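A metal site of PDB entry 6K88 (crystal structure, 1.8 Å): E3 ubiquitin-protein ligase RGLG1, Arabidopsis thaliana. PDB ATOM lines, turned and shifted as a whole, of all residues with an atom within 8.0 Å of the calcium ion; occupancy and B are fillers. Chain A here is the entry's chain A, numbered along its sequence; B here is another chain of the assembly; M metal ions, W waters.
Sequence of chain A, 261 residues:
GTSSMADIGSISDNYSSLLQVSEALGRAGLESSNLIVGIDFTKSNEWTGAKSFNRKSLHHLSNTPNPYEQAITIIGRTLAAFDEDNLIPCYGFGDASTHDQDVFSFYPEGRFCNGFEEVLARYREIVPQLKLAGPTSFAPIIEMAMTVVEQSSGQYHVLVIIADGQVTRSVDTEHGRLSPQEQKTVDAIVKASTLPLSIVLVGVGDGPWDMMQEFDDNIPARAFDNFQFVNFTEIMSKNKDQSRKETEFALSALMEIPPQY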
ATOM      1  N   SER A  33     -24.400  23.373  29.197  1.00  0.00           N
ATOM      2  CA  SER A  33     -25.669  23.527  28.487  1.00  0.00           C
ATOM      3  C   SER A  33     -26.155  24.974  28.402  1.00  0.00           C
ATOM      4  O   SER A  33     -25.586  25.878  29.010  1.00  0.00           O
ATOM      5  CB  SER A  33     -26.758  22.662  29.128  1.00  0.00           C
ATOM      6  OG  SER A  33     -26.879  22.944  30.509  1.00  0.00           O
ATOM      7  N   ASN A  34     -27.218  25.193  27.644  1.00  0.00           N
ATOM      8  CA  ASN A  34     -27.708  26.541  27.420  1.00  0.00           C
ATOM      9  C   ASN A  34     -29.239  26.526  27.331  1.00  0.00           C
ATOM     10  O   ASN A  34     -29.818  25.553  26.891  1.00  0.00           O
ATOM     11  CB  ASN A  34     -27.073  27.150  26.158  1.00  0.00           C
ATOM     12  CG  ASN A  34     -25.620  27.636  26.403  1.00  0.00           C
ATOM     13  OD1 ASN A  34     -25.372  28.608  27.156  1.00  0.00           O
ATOM     14  ND2 ASN A  34     -24.659  26.949  25.775  1.00  0.00           N
ATOM     15  N   LEU A  35     -29.859  27.590  27.827  1.00  0.00           N
ATOM     16  CA  LEU A  35     -31.311  27.672  27.984  1.00  0.00           C
ATOM     17  C   LEU A  35     -31.854  28.744  27.050  1.00  0.00           C
ATOM     18  O   LEU A  35     -31.346  29.857  27.031  1.00  0.00           O
ATOM     19  CB  LEU A  35     -31.672  28.012  29.437  1.00  0.00           C
ATOM     20  CG  LEU A  35     -33.076  27.952  30.042  1.00  0.00           C
ATOM     21  CD1 LEU A  35     -33.826  29.222  29.793  1.00  0.00           C
ATOM     22  CD2 LEU A  35     -33.869  26.784  29.505  1.00  0.00           C
ATOM     23  N   ILE A  36     -32.880  28.403  26.288  1.00  0.00           N
ATOM     24  CA  ILE A  36     -33.519  29.326  25.374  1.00  0.00           C
ATOM     25  C   ILE A  36     -34.956  29.562  25.832  1.00  0.00           C
ATOM     26  O   ILE A  36     -35.638  28.606  26.221  1.00  0.00           O
ATOM     27  CB  ILE A  36     -33.510  28.791  23.938  1.00  0.00           C
ATOM     28  CG1 ILE A  36     -32.094  28.446  23.481  1.00  0.00           C
ATOM     29  CG2 ILE A  36     -34.163  29.786  22.979  1.00  0.00           C
ATOM     30  CD1 ILE A  36     -32.084  27.422  22.366  1.00  0.00           C
ATOM     31  N   ALA A  80     -32.523  27.621  35.151  1.00  0.00           N
ATOM     32  CA  ALA A  80     -31.523  28.501  34.559  1.00  0.00           C
ATOM     33  C   ALA A  80     -30.165  28.377  35.243  1.00  0.00           C
ATOM     34  O   ALA A  80     -29.181  28.872  34.724  1.00  0.00           O
ATOM     35  CB  ALA A  80     -32.000  29.926  34.589  1.00  0.00           C
ATOM     36  N   PHE A  82     -28.396  25.898  35.305  1.00  0.00           N
ATOM     37  CA  PHE A  82     -27.531  25.084  34.443  1.00  0.00           C
ATOM     38  C   PHE A  82     -26.918  25.835  33.264  1.00  0.00           C
ATOM     39  O   PHE A  82     -25.965  25.359  32.655  1.00  0.00           O
ATOM     40  CB  PHE A  82     -28.287  23.870  33.893  1.00  0.00           C
ATOM     41  CG  PHE A  82     -28.578  22.828  34.926  1.00  0.00           C
ATOM     42  CD1 PHE A  82     -27.597  21.899  35.273  1.00  0.00           C
ATOM     43  CD2 PHE A  82     -29.809  22.771  35.560  1.00  0.00           C
ATOM     44  CE1 PHE A  82     -27.846  20.930  36.230  1.00  0.00           C
ATOM     45  CE2 PHE A  82     -30.073  21.803  36.500  1.00  0.00           C
ATOM     46  CZ  PHE A  82     -29.092  20.875  36.847  1.00  0.00           C
ATOM     47  N   ASP A  83     -27.485  26.992  32.926  1.00  0.00           N
ATOM     48  CA  ASP A  83     -27.019  27.704  31.746  1.00  0.00           C
ATOM     49  C   ASP A  83     -25.559  28.094  31.949  1.00  0.00           C
ATOM     50  O   ASP A  83     -25.228  28.744  32.928  1.00  0.00           O
ATOM     51  CB  ASP A  83     -27.880  28.951  31.466  1.00  0.00           C
ATOM     52  CG  ASP A  83     -27.508  29.633  30.173  1.00  0.00           C
ATOM     53  OD1 ASP A  83     -26.552  30.436  30.183  1.00  0.00           O
ATOM     54  OD2 ASP A  83     -28.143  29.363  29.126  1.00  0.00           O
ATOM     55  N   GLU A  84     -24.705  27.668  31.015  1.00  0.00           N
ATOM     56  CA  GLU A  84     -23.253  27.779  31.142  1.00  0.00           C
ATOM     57  C   GLU A  84     -22.753  29.223  31.322  1.00  0.00           C
ATOM     58  O   GLU A  84     -21.877  29.484  32.158  1.00  0.00           O
ATOM     59  CB  GLU A  84     -22.601  27.135  29.913  1.00  0.00           C
ATOM     60  CG  GLU A  84     -21.086  27.169  29.893  1.00  0.00           C
ATOM     61  CD  GLU A  84     -20.520  26.606  28.588  1.00  0.00           C
ATOM     62  OE1 GLU A  84     -20.914  27.083  27.501  1.00  0.00           O
ATOM     63  OE2 GLU A  84     -19.669  25.689  28.650  1.00  0.00           O
ATOM     64  N   ASP A  85     -23.284  30.173  30.554  1.00  0.00           N
ATOM     65  CA  ASP A  85     -22.794  31.552  30.671  1.00  0.00           C
ATOM     66  C   ASP A  85     -23.781  32.567  31.243  1.00  0.00           C
ATOM     67  O   ASP A  85     -23.431  33.742  31.346  1.00  0.00           O
ATOM     68  CB  ASP A  85     -22.303  32.064  29.315  1.00  0.00           C
ATOM     69  CG  ASP A  85     -23.342  31.947  28.208  1.00  0.00           C
ATOM     70  OD1 ASP A  85     -24.548  31.739  28.494  1.00  0.00           O
ATOM     71  OD2 ASP A  85     -22.946  32.092  27.039  1.00  0.00           O
ATOM     72  N   ASN A  86     -24.983  32.137  31.614  1.00  0.00           N
ATOM     73  CA  ASN A  86     -26.021  33.031  32.158  1.00  0.00           C
ATOM     74  C   ASN A  86     -26.494  34.057  31.135  1.00  0.00           C
ATOM     75  O   ASN A  86     -27.121  35.052  31.486  1.00  0.00           O
ATOM     76  CB  ASN A  86     -25.548  33.765  33.422  1.00  0.00           C
ATOM     77  CG  ASN A  86     -26.682  34.128  34.331  1.00  0.00           C
ATOM     78  OD1 ASN A  86     -27.732  33.485  34.308  1.00  0.00           O
ATOM     79  ND2 ASN A  86     -26.501  35.170  35.139  1.00  0.00           N
ATOM     80  N   LEU A  87     -26.188  33.797  29.875  1.00  0.00           N
ATOM     81  CA  LEU A  87     -26.719  34.609  28.783  1.00  0.00           C
ATOM     82  C   LEU A  87     -27.846  33.823  28.127  1.00  0.00           C
ATOM     83  O   LEU A  87     -27.661  32.682  27.710  1.00  0.00           O
ATOM     84  CB  LEU A  87     -25.617  34.941  27.774  1.00  0.00           C
ATOM     85  CG  LEU A  87     -24.437  35.703  28.400  1.00  0.00           C
ATOM     86  CD1 LEU A  87     -23.349  35.984  27.380  1.00  0.00           C
ATOM     87  CD2 LEU A  87     -24.915  37.001  29.042  1.00  0.00           C
ATOM     88  N   ILE A  88     -29.027  34.447  28.040  1.00  0.00           N
ATOM     89  CA  ILE A  88     -30.250  33.715  27.693  1.00  0.00           C
ATOM     90  C   ILE A  88     -30.943  34.300  26.467  1.00  0.00           C
ATOM     91  O   ILE A  88     -31.480  35.407  26.539  1.00  0.00           O
ATOM     92  CB  ILE A  88     -31.272  33.751  28.863  1.00  0.00           C
ATOM     93  CG1 ILE A  88     -30.589  33.513  30.212  1.00  0.00           C
ATOM     94  CG2 ILE A  88     -32.440  32.757  28.594  1.00  0.00           C
ATOM     95  CD1 ILE A  88     -30.053  32.093  30.405  1.00  0.00           C
ATOM     96  N   PRO A  89     -30.919  33.565  25.342  1.00  0.00           N
ATOM     97  CA  PRO A  89     -31.675  34.022  24.170  1.00  0.00           C
ATOM     98  C   PRO A  89     -33.144  34.031  24.535  1.00  0.00           C
ATOM     99  O   PRO A  89     -33.616  33.008  25.027  1.00  0.00           O
ATOM    100  CB  PRO A  89     -31.355  32.958  23.096  1.00  0.00           C
ATOM    101  CG  PRO A  89     -30.136  32.226  23.620  1.00  0.00           C
ATOM    102  CD  PRO A  89     -30.237  32.292  25.109  1.00  0.00           C
ATOM    103  N   PHE A 112     -28.462  38.638  23.621  1.00  0.00           N
ATOM    104  CA  PHE A 112     -29.063  37.757  24.614  1.00  0.00           C
ATOM    105  C   PHE A 112     -29.300  38.498  25.932  1.00  0.00           C
ATOM    106  O   PHE A 112     -28.573  39.427  26.263  1.00  0.00           O
ATOM    107  CB  PHE A 112     -28.177  36.536  24.888  1.00  0.00           C
ATOM    108  CG  PHE A 112     -27.969  35.643  23.686  1.00  0.00           C
ATOM    109  CD1 PHE A 112     -28.776  35.732  22.572  1.00  0.00           C
ATOM    110  CD2 PHE A 112     -26.953  34.690  23.696  1.00  0.00           C
ATOM    111  CE1 PHE A 112     -28.570  34.904  21.468  1.00  0.00           C
ATOM    112  CE2 PHE A 112     -26.734  33.853  22.604  1.00  0.00           C
ATOM    113  CZ  PHE A 112     -27.539  33.958  21.484  1.00  0.00           C
ATOM    114  N   CYS A 113     -30.322  38.081  26.678  1.00  0.00           N
ATOM    115  CA  CYS A 113     -30.557  38.608  28.018  1.00  0.00           C
ATOM    116  C   CYS A 113     -29.440  38.193  28.969  1.00  0.00           C
ATOM    117  O   CYS A 113     -28.941  37.061  28.905  1.00  0.00           O
ATOM    118  CB  CYS A 113     -31.895  38.115  28.572  1.00  0.00           C
ATOM    119  SG  CYS A 113     -33.352  38.799  27.750  1.00  0.00           S
ATOM    120  N   VAL A 148     -30.340  28.533  16.791  1.00  0.00           N
ATOM    121  CA  VAL A 148     -29.436  28.761  17.909  1.00  0.00           C
ATOM    122  C   VAL A 148     -28.575  27.514  18.207  1.00  0.00           C
ATOM    123  O   VAL A 148     -27.368  27.636  18.441  1.00  0.00           O
ATOM    124  CB  VAL A 148     -30.216  29.166  19.188  1.00  0.00           C
ATOM    125  CG1 VAL A 148     -29.312  29.131  20.414  1.00  0.00           C
ATOM    126  CG2 VAL A 148     -30.843  30.540  19.009  1.00  0.00           C
ATOM    127  N   HIS A 157     -29.027  21.910  24.666  1.00  0.00           N
ATOM    128  CA  HIS A 157     -29.906  23.056  24.807  1.00  0.00           C
ATOM    129  C   HIS A 157     -31.266  22.632  25.322  1.00  0.00           C
ATOM    130  O   HIS A 157     -31.754  21.558  24.988  1.00  0.00           O
ATOM    131  CB  HIS A 157     -30.065  23.784  23.459  1.00  0.00           C
ATOM    132  CG  HIS A 157     -28.837  24.504  23.008  1.00  0.00           C
ATOM    133  ND1 HIS A 157     -28.722  25.880  23.034  1.00  0.00           N
ATOM    134  CD2 HIS A 157     -27.673  24.039  22.496  1.00  0.00           C
ATOM    135  CE1 HIS A 157     -27.540  26.235  22.565  1.00  0.00           C
ATOM    136  NE2 HIS A 157     -26.883  25.138  22.230  1.00  0.00           N
ATOM    137  N   ARG B 244     -26.439  30.086  42.182  1.00  0.00           N
ATOM    138  CA  ARG B 244     -26.710  29.290  40.981  1.00  0.00           C
ATOM    139  C   ARG B 244     -25.975  27.956  41.046  1.00  0.00           C
ATOM    140  O   ARG B 244     -26.503  26.927  40.638  1.00  0.00           O
ATOM    141  CB  ARG B 244     -26.321  30.048  39.699  1.00  0.00           C
ATOM    142  CG  ARG B 244     -27.210  31.290  39.449  1.00  0.00           C
ATOM    143  CD  ARG B 244     -26.906  31.998  38.136  1.00  0.00           C
ATOM    144  NE  ARG B 244     -27.209  31.172  36.964  1.00  0.00           N
ATOM    145  CZ  ARG B 244     -26.309  30.826  36.046  1.00  0.00           C
ATOM    146  NH1 ARG B 244     -25.055  31.246  36.147  1.00  0.00           N
ATOM    147  NH2 ARG B 244     -26.668  30.073  35.027  1.00  0.00           N
HETATM  148 CA    CA M   1     -26.525  30.644  27.687  1.00  0.00          CA
HETATM  149  O   HOH W   1     -27.992  29.844  25.997  1.00  0.00           O
HETATM  150  O   HOH W   2     -25.622  31.315  25.538  1.00  0.00           O
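The backbone NH (N) of Asn 86 sits close to the side-chain carboxylate (OD1) of Asp 83 (2.7 Å).
The backbone NH (N) of Leu 35 sits close to the side-chain carboxylate (OD2) of Asp 83 (2.8 Å).
The guanidinium group of Arg 244 of chain B is in hydrogen-bond range of the backbone carbonyl oxygen of Asp 83 (2.9 Å).
The backbone carbonyl oxygen (O) of Leu 87 is bound to the calcium ion.
The calcium ion is bound by water W1 (2.4 Å).
OD1 of Asn 34 is bound to the calcium ion (2.4 Å).
OD1 of Asp 85 is bound to the calcium ion.
Water W2 is bound to the calcium ion, 2.4 Å away.
OD1 of Asp 83 binds the calcium ion (2.5 Å).
OD2 of Asp 83 binds the calcium ion.
The calcium ion has seven donor atoms within binding distance.
Four residues have an atom within 4 Å of the calcium ion: Asn 34, Asp 83, Asp 85 and Leu 87.
The nearest printed residue that does not touch the calcium ion is Asn 86 (4.5 Å).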
